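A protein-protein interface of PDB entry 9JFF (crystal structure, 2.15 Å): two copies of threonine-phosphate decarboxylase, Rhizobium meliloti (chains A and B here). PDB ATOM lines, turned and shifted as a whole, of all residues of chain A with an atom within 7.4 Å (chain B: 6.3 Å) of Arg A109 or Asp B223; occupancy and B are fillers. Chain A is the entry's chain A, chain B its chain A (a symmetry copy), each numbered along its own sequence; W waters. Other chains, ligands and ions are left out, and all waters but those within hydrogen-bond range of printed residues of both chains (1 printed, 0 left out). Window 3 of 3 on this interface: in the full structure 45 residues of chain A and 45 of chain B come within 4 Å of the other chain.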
ATOM      1  N   ALA A   3      -4.044  -7.591 -25.775  1.00  0.00           N
ATOM      2  CA  ALA A   3      -4.898  -6.674 -26.529  1.00  0.00           C
ATOM      3  C   ALA A   3      -5.489  -5.578 -25.638  1.00  0.00           C
ATOM      4  O   ALA A   3      -5.869  -5.835 -24.492  1.00  0.00           O
ATOM      5  CB  ALA A   3      -6.012  -7.444 -27.233  1.00  0.00           C
ATOM      6  N   PRO A   4      -5.565  -4.355 -26.165  1.00  0.00           N
ATOM      7  CA  PRO A   4      -6.125  -3.252 -25.377  1.00  0.00           C
ATOM      8  C   PRO A   4      -7.629  -3.392 -25.188  1.00  0.00           C
ATOM      9  O   PRO A   4      -8.331  -3.988 -26.010  1.00  0.00           O
ATOM     10  CB  PRO A   4      -5.779  -2.009 -26.209  1.00  0.00           C
ATOM     11  CG  PRO A   4      -5.622  -2.515 -27.605  1.00  0.00           C
ATOM     12  CD  PRO A   4      -5.071  -3.909 -27.483  1.00  0.00           C
ATOM     13  N   ILE A   5      -8.113  -2.833 -24.072  1.00  0.00           N
ATOM     14  CA  ILE A   5      -9.537  -2.837 -23.754  1.00  0.00           C
ATOM     15  C   ILE A   5     -10.338  -2.271 -24.921  1.00  0.00           C
ATOM     16  O   ILE A   5      -9.934  -1.293 -25.563  1.00  0.00           O
ATOM     17  CB  ILE A   5      -9.784  -2.020 -22.471  1.00  0.00           C
ATOM     18  CG1 ILE A   5      -9.142  -2.698 -21.258  1.00  0.00           C
ATOM     19  CG2 ILE A   5     -11.274  -1.758 -22.251  1.00  0.00           C
ATOM     20  CD1 ILE A   5      -9.009  -1.775 -20.058  1.00  0.00           C
ATOM     21  N   VAL A   6     -11.487  -2.883 -25.197  1.00  0.00           N
ATOM     22  CA  VAL A   6     -12.406  -2.365 -26.214  1.00  0.00           C
ATOM     23  C   VAL A   6     -13.325  -1.372 -25.506  1.00  0.00           C
ATOM     24  O   VAL A   6     -14.377  -1.725 -24.971  1.00  0.00           O
ATOM     25  CB  VAL A   6     -13.179  -3.478 -26.918  1.00  0.00           C
ATOM     26  CG1 VAL A   6     -14.081  -2.883 -28.006  1.00  0.00           C
ATOM     27  CG2 VAL A   6     -12.218  -4.493 -27.524  1.00  0.00           C
ATOM     28  N   HIS A   7     -12.913  -0.108 -25.501  1.00  0.00           N
ATOM     29  CA  HIS A   7     -13.719   0.960 -24.935  1.00  0.00           C
ATOM     30  C   HIS A   7     -14.876   1.305 -25.865  1.00  0.00           C
ATOM     31  O   HIS A   7     -14.879   0.958 -27.048  1.00  0.00           O
ATOM     32  CB  HIS A   7     -12.866   2.208 -24.705  1.00  0.00           C
ATOM     33  CG  HIS A   7     -11.745   2.001 -23.736  1.00  0.00           C
ATOM     34  ND1 HIS A   7     -11.953   1.833 -22.384  1.00  0.00           N
ATOM     35  CD2 HIS A   7     -10.405   1.935 -23.922  1.00  0.00           C
ATOM     36  CE1 HIS A   7     -10.789   1.668 -21.779  1.00  0.00           C
ATOM     37  NE2 HIS A   7      -9.834   1.733 -22.689  1.00  0.00           N
ATOM     38  N   GLN A  81      -6.662  10.025 -19.007  1.00  0.00           N
ATOM     39  CA  GLN A  81      -5.940   8.815 -19.376  1.00  0.00           C
ATOM     40  C   GLN A  81      -4.435   9.006 -19.230  1.00  0.00           C
ATOM     41  O   GLN A  81      -3.722   8.086 -18.814  1.00  0.00           O
ATOM     42  CB  GLN A  81      -6.289   8.409 -20.808  1.00  0.00           C
ATOM     43  CG  GLN A  81      -5.799   7.011 -21.156  1.00  0.00           C
ATOM     44  CD  GLN A  81      -6.382   5.959 -20.221  1.00  0.00           C
ATOM     45  OE1 GLN A  81      -7.570   6.005 -19.881  1.00  0.00           O
ATOM     46  NE2 GLN A  81      -5.547   5.021 -19.789  1.00  0.00           N
ATOM     47  N   ILE A  84      -3.642   8.599 -15.624  1.00  0.00           N
ATOM     48  CA  ILE A  84      -3.831   7.198 -15.247  1.00  0.00           C
ATOM     49  C   ILE A  84      -2.587   6.389 -15.606  1.00  0.00           C
ATOM     50  O   ILE A  84      -2.046   5.658 -14.768  1.00  0.00           O
ATOM     51  CB  ILE A  84      -5.096   6.615 -15.902  1.00  0.00           C
ATOM     52  CG1 ILE A  84      -6.350   7.321 -15.385  1.00  0.00           C
ATOM     53  CG2 ILE A  84      -5.199   5.122 -15.600  1.00  0.00           C
ATOM     54  CD1 ILE A  84      -7.635   6.886 -16.084  1.00  0.00           C
ATOM     55  N   GLN A  85      -2.092   6.540 -16.851  1.00  0.00           N
ATOM     56  CA  GLN A  85      -0.844   5.895 -17.270  1.00  0.00           C
ATOM     57  C   GLN A  85       0.314   6.162 -16.307  1.00  0.00           C
ATOM     58  O   GLN A  85       1.281   5.394 -16.294  1.00  0.00           O
ATOM     59  CB  GLN A  85      -0.404   6.355 -18.675  1.00  0.00           C
ATOM     60  CG  GLN A  85      -1.414   6.215 -19.836  1.00  0.00           C
ATOM     61  CD  GLN A  85      -1.587   4.788 -20.346  1.00  0.00           C
ATOM     62  OE1 GLN A  85      -2.707   4.354 -20.626  1.00  0.00           O
ATOM     63  NE2 GLN A  85      -0.484   4.057 -20.480  1.00  0.00           N
ATOM     64  N   ILE A  99      -9.355  -1.026  -5.752  1.00  0.00           N
ATOM     65  CA  ILE A  99     -10.181  -0.322  -6.729  1.00  0.00           C
ATOM     66  C   ILE A  99     -11.641  -0.672  -6.465  1.00  0.00           C
ATOM     67  O   ILE A  99     -12.020  -1.850  -6.500  1.00  0.00           O
ATOM     68  CB  ILE A  99      -9.779  -0.671  -8.172  1.00  0.00           C
ATOM     69  CG1 ILE A  99      -8.294  -0.378  -8.401  1.00  0.00           C
ATOM     70  CG2 ILE A  99     -10.640   0.105  -9.168  1.00  0.00           C
ATOM     71  CD1 ILE A  99      -7.828  -0.659  -9.810  1.00  0.00           C
ATOM     72  N   TYR A 104     -14.194   1.552 -14.609  1.00  0.00           N
ATOM     73  CA  TYR A 104     -13.334   1.826 -15.756  1.00  0.00           C
ATOM     74  C   TYR A 104     -12.069   0.972 -15.687  1.00  0.00           C
ATOM     75  O   TYR A 104     -11.392   0.923 -14.656  1.00  0.00           O
ATOM     76  CB  TYR A 104     -12.999   3.319 -15.774  1.00  0.00           C
ATOM     77  CG  TYR A 104     -12.263   3.788 -16.997  1.00  0.00           C
ATOM     78  CD1 TYR A 104     -12.819   3.647 -18.270  1.00  0.00           C
ATOM     79  CD2 TYR A 104     -11.019   4.401 -16.881  1.00  0.00           C
ATOM     80  CE1 TYR A 104     -12.138   4.084 -19.397  1.00  0.00           C
ATOM     81  CE2 TYR A 104     -10.338   4.847 -17.995  1.00  0.00           C
ATOM     82  CZ  TYR A 104     -10.896   4.684 -19.253  1.00  0.00           C
ATOM     83  OH  TYR A 104     -10.207   5.135 -20.358  1.00  0.00           O
ATOM     84  N   GLY A 105     -11.781   0.260 -16.780  1.00  0.00           N
ATOM     85  CA  GLY A 105     -10.807  -0.817 -16.731  1.00  0.00           C
ATOM     86  C   GLY A 105      -9.349  -0.408 -16.793  1.00  0.00           C
ATOM     87  O   GLY A 105      -8.481  -1.241 -16.522  1.00  0.00           O
ATOM     88  N   GLU A 106      -9.051   0.847 -17.137  1.00  0.00           N
ATOM     89  CA  GLU A 106      -7.660   1.222 -17.372  1.00  0.00           C
ATOM     90  C   GLU A 106      -6.857   1.279 -16.078  1.00  0.00           C
ATOM     91  O   GLU A 106      -5.638   1.081 -16.103  1.00  0.00           O
ATOM     92  CB  GLU A 106      -7.597   2.561 -18.107  1.00  0.00           C
ATOM     93  CG  GLU A 106      -8.035   2.481 -19.573  1.00  0.00           C
ATOM     94  CD  GLU A 106      -7.020   1.760 -20.453  1.00  0.00           C
ATOM     95  OE1 GLU A 106      -5.854   1.621 -20.023  1.00  0.00           O
ATOM     96  OE2 GLU A 106      -7.387   1.336 -21.574  1.00  0.00           O
ATOM     97  N   TYR A 107      -7.514   1.536 -14.944  1.00  0.00           N
ATOM     98  CA  TYR A 107      -6.802   1.580 -13.669  1.00  0.00           C
ATOM     99  C   TYR A 107      -6.131   0.249 -13.362  1.00  0.00           C
ATOM    100  O   TYR A 107      -4.924   0.195 -13.093  1.00  0.00           O
ATOM    101  CB  TYR A 107      -7.760   1.973 -12.547  1.00  0.00           C
ATOM    102  CG  TYR A 107      -8.156   3.423 -12.620  1.00  0.00           C
ATOM    103  CD1 TYR A 107      -7.244   4.420 -12.285  1.00  0.00           C
ATOM    104  CD2 TYR A 107      -9.428   3.804 -13.039  1.00  0.00           C
ATOM    105  CE1 TYR A 107      -7.583   5.756 -12.360  1.00  0.00           C
ATOM    106  CE2 TYR A 107      -9.784   5.149 -13.112  1.00  0.00           C
ATOM    107  CZ  TYR A 107      -8.853   6.116 -12.775  1.00  0.00           C
ATOM    108  OH  TYR A 107      -9.180   7.453 -12.838  1.00  0.00           O
ATOM    109  N   ALA A 108      -6.896  -0.842 -13.397  1.00  0.00           N
ATOM    110  CA  ALA A 108      -6.308  -2.149 -13.129  1.00  0.00           C
ATOM    111  C   ALA A 108      -5.330  -2.555 -14.230  1.00  0.00           C
ATOM    112  O   ALA A 108      -4.300  -3.181 -13.951  1.00  0.00           O
ATOM    113  CB  ALA A 108      -7.412  -3.199 -12.968  1.00  0.00           C
ATOM    114  N   ARG A 109      -5.635  -2.214 -15.485  1.00  0.00           N
ATOM    115  CA  ARG A 109      -4.756  -2.606 -16.583  1.00  0.00           C
ATOM    116  C   ARG A 109      -3.382  -1.968 -16.428  1.00  0.00           C
ATOM    117  O   ARG A 109      -2.352  -2.648 -16.502  1.00  0.00           O
ATOM    118  CB  ARG A 109      -5.375  -2.217 -17.930  1.00  0.00           C
ATOM    119  CG  ARG A 109      -4.440  -2.478 -19.114  1.00  0.00           C
ATOM    120  CD  ARG A 109      -4.936  -1.863 -20.414  1.00  0.00           C
ATOM    121  NE  ARG A 109      -3.990  -2.082 -21.507  1.00  0.00           N
ATOM    122  CZ  ARG A 109      -4.005  -3.132 -22.320  1.00  0.00           C
ATOM    123  NH1 ARG A 109      -4.930  -4.077 -22.218  1.00  0.00           N
ATOM    124  NH2 ARG A 109      -3.068  -3.241 -23.260  1.00  0.00           N
ATOM    125  N   VAL A 110      -3.355  -0.654 -16.200  1.00  0.00           N
ATOM    126  CA  VAL A 110      -2.091   0.063 -16.068  1.00  0.00           C
ATOM    127  C   VAL A 110      -1.332  -0.419 -14.834  1.00  0.00           C
ATOM    128  O   VAL A 110      -0.131  -0.709 -14.895  1.00  0.00           O
ATOM    129  CB  VAL A 110      -2.349   1.581 -16.023  1.00  0.00           C
ATOM    130  CG1 VAL A 110      -1.114   2.322 -15.566  1.00  0.00           C
ATOM    131  CG2 VAL A 110      -2.798   2.074 -17.397  1.00  0.00           C
ATOM    132  N   LEU A 111      -2.022  -0.527 -13.698  1.00  0.00           N
ATOM    133  CA  LEU A 111      -1.311  -0.822 -12.460  1.00  0.00           C
ATOM    134  C   LEU A 111      -0.799  -2.260 -12.433  1.00  0.00           C
ATOM    135  O   LEU A 111       0.316  -2.512 -11.960  1.00  0.00           O
ATOM    136  CB  LEU A 111      -2.203  -0.525 -11.258  1.00  0.00           C
ATOM    137  CG  LEU A 111      -2.323   0.977 -10.982  1.00  0.00           C
ATOM    138  CD1 LEU A 111      -3.588   1.289 -10.208  1.00  0.00           C
ATOM    139  CD2 LEU A 111      -1.094   1.502 -10.237  1.00  0.00           C
ATOM    140  N   GLU A 112      -1.582  -3.216 -12.943  1.00  0.00           N
ATOM    141  CA  GLU A 112      -1.108  -4.598 -12.966  1.00  0.00           C
ATOM    142  C   GLU A 112       0.039  -4.766 -13.954  1.00  0.00           C
ATOM    143  O   GLU A 112       0.974  -5.532 -13.700  1.00  0.00           O
ATOM    144  CB  GLU A 112      -2.257  -5.559 -13.288  1.00  0.00           C
ATOM    145  CG  GLU A 112      -3.296  -5.651 -12.154  1.00  0.00           C
ATOM    146  CD  GLU A 112      -4.424  -6.638 -12.429  1.00  0.00           C
ATOM    147  OE1 GLU A 112      -4.757  -6.862 -13.614  1.00  0.00           O
ATOM    148  OE2 GLU A 112      -4.978  -7.197 -11.455  1.00  0.00           O
ATOM    149  N   ALA A 113      -0.003  -4.043 -15.076  1.00  0.00           N
ATOM    150  CA  ALA A 113       1.113  -4.082 -16.013  1.00  0.00           C
ATOM    151  C   ALA A 113       2.394  -3.564 -15.371  1.00  0.00           C
ATOM    152  O   ALA A 113       3.490  -3.967 -15.765  1.00  0.00           O
ATOM    153  CB  ALA A 113       0.780  -3.277 -17.272  1.00  0.00           C
ATOM    154  N   ALA A 114       2.278  -2.687 -14.378  1.00  0.00           N
ATOM    155  CA  ALA A 114       3.436  -2.164 -13.668  1.00  0.00           C
ATOM    156  C   ALA A 114       3.828  -3.013 -12.465  1.00  0.00           C
ATOM    157  O   ALA A 114       4.648  -2.568 -11.657  1.00  0.00           O
ATOM    158  CB  ALA A 114       3.178  -0.724 -13.219  1.00  0.00           C
ATOM    159  N   GLY A 115       3.248  -4.206 -12.316  1.00  0.00           N
ATOM    160  CA  GLY A 115       3.613  -5.107 -11.238  1.00  0.00           C
ATOM    161  C   GLY A 115       2.909  -4.884  -9.916  1.00  0.00           C
ATOM    162  O   GLY A 115       3.291  -5.509  -8.922  1.00  0.00           O
ATOM    163  N   VAL A 118      -3.578  -5.694  -7.444  1.00  0.00           N
ATOM    164  CA  VAL A 118      -4.819  -4.924  -7.444  1.00  0.00           C
ATOM    165  C   VAL A 118      -5.913  -5.746  -6.773  1.00  0.00           C
ATOM    166  O   VAL A 118      -6.180  -6.885  -7.174  1.00  0.00           O
ATOM    167  CB  VAL A 118      -5.230  -4.513  -8.871  1.00  0.00           C
ATOM    168  CG1 VAL A 118      -6.637  -3.924  -8.875  1.00  0.00           C
ATOM    169  CG2 VAL A 118      -4.250  -3.506  -9.426  1.00  0.00           C
ATOM    170  N   ARG B  89      11.794   3.582 -20.961  1.00  0.00           N
ATOM    171  CA  ARG B  89      11.188   2.259 -21.097  1.00  0.00           C
ATOM    172  C   ARG B  89      11.723   1.507 -22.309  1.00  0.00           C
ATOM    173  O   ARG B  89      11.629   0.276 -22.355  1.00  0.00           O
ATOM    174  CB  ARG B  89       9.663   2.397 -21.173  1.00  0.00           C
ATOM    175  CG  ARG B  89       9.114   3.441 -20.195  1.00  0.00           C
ATOM    176  CD  ARG B  89       7.586   3.483 -20.145  1.00  0.00           C
ATOM    177  NE  ARG B  89       7.040   2.243 -19.612  1.00  0.00           N
ATOM    178  CZ  ARG B  89       5.797   2.088 -19.177  1.00  0.00           C
ATOM    179  NH1 ARG B  89       4.934   3.093 -19.166  1.00  0.00           N
ATOM    180  NH2 ARG B  89       5.411   0.892 -18.743  1.00  0.00           N
ATOM    181  N   LEU B 218       6.704   0.326 -32.441  1.00  0.00           N
ATOM    182  CA  LEU B 218       5.507   1.161 -32.522  1.00  0.00           C
ATOM    183  C   LEU B 218       4.402   0.635 -31.611  1.00  0.00           C
ATOM    184  O   LEU B 218       3.699   1.419 -30.960  1.00  0.00           O
ATOM    185  CB  LEU B 218       5.014   1.244 -33.969  1.00  0.00           C
ATOM    186  CG  LEU B 218       5.933   1.927 -34.990  1.00  0.00           C
ATOM    187  CD1 LEU B 218       5.266   1.954 -36.367  1.00  0.00           C
ATOM    188  CD2 LEU B 218       6.318   3.330 -34.534  1.00  0.00           C
ATOM    189  N   ALA B 219       4.238  -0.691 -31.547  1.00  0.00           N
ATOM    190  CA  ALA B 219       3.227  -1.256 -30.654  1.00  0.00           C
ATOM    191  C   ALA B 219       3.549  -0.950 -29.199  1.00  0.00           C
ATOM    192  O   ALA B 219       2.642  -0.699 -28.397  1.00  0.00           O
ATOM    193  CB  ALA B 219       3.103  -2.766 -30.872  1.00  0.00           C
ATOM    194  N   SER B 220       4.837  -0.940 -28.838  1.00  0.00           N
ATOM    195  CA  SER B 220       5.207  -0.595 -27.468  1.00  0.00           C
ATOM    196  C   SER B 220       4.871   0.857 -27.152  1.00  0.00           C
ATOM    197  O   SER B 220       4.272   1.150 -26.111  1.00  0.00           O
ATOM    198  CB  SER B 220       6.694  -0.870 -27.231  1.00  0.00           C
ATOM    199  OG  SER B 220       6.986  -2.235 -27.448  1.00  0.00           O
ATOM    200  N   PHE B 221       5.271   1.788 -28.026  1.00  0.00           N
ATOM    201  CA  PHE B 221       4.943   3.195 -27.796  1.00  0.00           C
ATOM    202  C   PHE B 221       3.434   3.401 -27.696  1.00  0.00           C
ATOM    203  O   PHE B 221       2.958   4.161 -26.846  1.00  0.00           O
ATOM    204  CB  PHE B 221       5.513   4.073 -28.914  1.00  0.00           C
ATOM    205  CG  PHE B 221       6.951   4.468 -28.722  1.00  0.00           C
ATOM    206  CD1 PHE B 221       7.324   5.298 -27.676  1.00  0.00           C
ATOM    207  CD2 PHE B 221       7.925   4.037 -29.613  1.00  0.00           C
ATOM    208  CE1 PHE B 221       8.650   5.681 -27.505  1.00  0.00           C
ATOM    209  CE2 PHE B 221       9.252   4.413 -29.451  1.00  0.00           C
ATOM    210  CZ  PHE B 221       9.614   5.240 -28.394  1.00  0.00           C
ATOM    211  N   ALA B 222       2.670   2.737 -28.566  1.00  0.00           N
ATOM    212  CA  ALA B 222       1.218   2.888 -28.552  1.00  0.00           C
ATOM    213  C   ALA B 222       0.629   2.426 -27.223  1.00  0.00           C
ATOM    214  O   ALA B 222      -0.267   3.080 -26.672  1.00  0.00           O
ATOM    215  CB  ALA B 222       0.600   2.112 -29.717  1.00  0.00           C
ATOM    216  N   ASP B 223       1.134   1.313 -26.683  1.00  0.00           N
ATOM    217  CA  ASP B 223       0.624   0.822 -25.406  1.00  0.00           C
ATOM    218  C   ASP B 223       0.988   1.763 -24.266  1.00  0.00           C
ATOM    219  O   ASP B 223       0.146   2.067 -23.413  1.00  0.00           O
ATOM    220  CB  ASP B 223       1.156  -0.586 -25.129  1.00  0.00           C
ATOM    221  CG  ASP B 223       0.596  -1.175 -23.838  1.00  0.00           C
ATOM    222  OD1 ASP B 223      -0.603  -1.538 -23.813  1.00  0.00           O
ATOM    223  OD2 ASP B 223       1.355  -1.264 -22.849  1.00  0.00           O
ATOM    224  N   TRP B 224       2.232   2.255 -24.251  1.00  0.00           N
ATOM    225  CA  TRP B 224       2.671   3.159 -23.191  1.00  0.00           C
ATOM    226  C   TRP B 224       1.873   4.457 -23.192  1.00  0.00           C
ATOM    227  O   TRP B 224       1.595   5.026 -22.128  1.00  0.00           O
ATOM    228  CB  TRP B 224       4.161   3.467 -23.352  1.00  0.00           C
ATOM    229  CG  TRP B 224       5.063   2.280 -23.216  1.00  0.00           C
ATOM    230  CD1 TRP B 224       4.830   1.150 -22.489  1.00  0.00           C
ATOM    231  CD2 TRP B 224       6.348   2.106 -23.829  1.00  0.00           C
ATOM    232  NE1 TRP B 224       5.892   0.286 -22.608  1.00  0.00           N
ATOM    233  CE2 TRP B 224       6.837   0.849 -23.424  1.00  0.00           C
ATOM    234  CE3 TRP B 224       7.136   2.895 -24.676  1.00  0.00           C
ATOM    235  CZ2 TRP B 224       8.079   0.359 -23.841  1.00  0.00           C
ATOM    236  CZ3 TRP B 224       8.365   2.405 -25.091  1.00  0.00           C
ATOM    237  CH2 TRP B 224       8.828   1.154 -24.669  1.00  0.00           C
ATOM    238  N   LEU B 225       1.520   4.959 -24.379  1.00  0.00           N
ATOM    239  CA  LEU B 225       0.801   6.225 -24.461  1.00  0.00           C
ATOM    240  C   LEU B 225      -0.670   6.080 -24.086  1.00  0.00           C
ATOM    241  O   LEU B 225      -1.280   7.047 -23.620  1.00  0.00           O
ATOM    242  CB  LEU B 225       0.933   6.808 -25.870  1.00  0.00           C
ATOM    243  CG  LEU B 225       2.324   7.355 -26.199  1.00  0.00           C
ATOM    244  CD1 LEU B 225       2.504   7.511 -27.691  1.00  0.00           C
ATOM    245  CD2 LEU B 225       2.541   8.690 -25.496  1.00  0.00           C
ATOM    246  N   GLY B 226      -1.257   4.902 -24.294  1.00  0.00           N
ATOM    247  CA  GLY B 226      -2.635   4.669 -23.925  1.00  0.00           C
ATOM    248  C   GLY B 226      -3.613   5.154 -24.977  1.00  0.00           C
ATOM    249  O   GLY B 226      -3.231   5.790 -25.964  1.00  0.00           O
ATOM    250  N   PRO B 227      -4.901   4.862 -24.782  1.00  0.00           N
ATOM    251  CA  PRO B 227      -5.902   5.207 -25.802  1.00  0.00           C
ATOM    252  C   PRO B 227      -6.110   6.711 -25.929  1.00  0.00           C
ATOM    253  O   PRO B 227      -5.943   7.469 -24.970  1.00  0.00           O
ATOM    254  CB  PRO B 227      -7.174   4.518 -25.293  1.00  0.00           C
ATOM    255  CG  PRO B 227      -6.980   4.436 -23.804  1.00  0.00           C
ATOM    256  CD  PRO B 227      -5.502   4.188 -23.617  1.00  0.00           C
HETATM  257  O   HOH W   1       1.830   3.164 -17.813  1.00  0.00           O
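CD of Pro B227 touches CG of Gln A81 (3.8 Å).
Gln A85 touches Asp B223.
O of Leu B225 touches CG of Gln A85 (3.9 Å).
Gln A85 touches Gly B226.
CG of Pro B227 touches OE2 of Glu A106, 3.8 Å away.
No residue of chain A comes within 4 Å of Ala B222.
Of the printed residues of chain A, Asp B223 touches Gln A85 (3.6 Å) and Arg A109 (3.0 Å).
Of the printed residues of chain A, Gly B226 touches Gln A85.
Of the printed residues of chain A, Pro B227 touches Gln A81 and Glu A106.
The nearest printed residue of chain B that does not touch Arg A109 is Pro B227 (6.8 Å).
The nearest residue of chain A that does not touch Asp B223 is Pro A4 (5.7 Å).
The nearest printed residue of chain B that does not touch Glu A106 is Gly B226 (5.9 Å).
No position is printed for both chains.
The backbone carbonyl oxygen of Ala A3 lies within hydrogen-bond range of the guanidinium group of Arg A109, at 3.0 Å.
The side-chain carboxylate (OE2) of Glu A106 sits at hydrogen-bond distance from a ring nitrogen (NE2) of His A7, at 2.7 Å.
NE2 of Gln A81 lies within hydrogen-bond range of OE1 of Gln A85, 3.0 Å away.
OE1 of Gln A81 is in hydrogen-bond range of OH of Tyr A104 (2.8 Å).
OE1 of Glu A106 sits at hydrogen-bond distance from NE2 of Gln A81, 3.4 Å away.
Water W1 bridges O of Gln A85 (2.8 Å) and NH1 of Arg B89 (3.4 Å).
Of the 22 printed residues of chain A, 4 touch a printed residue of chain B.
Of the 11 printed residues of chain B, 5 touch a printed residue of chain A.
Hydrophobic or aromatic side chains of chain B within 4 Å of the printed part of chain A: Pro B227.
Along chain B the printed residues that touch a printed residue of chain A span positions 223 to 227.
The side-chain amide nitrogen (NE2) of Gln A85 sits at hydrogen-bond distance from the backbone carbonyl oxygen (O) of Trp B224.
NH2 of Arg A109 is in salt-bridge range of OD1 of Asp B223 (3.0 Å).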
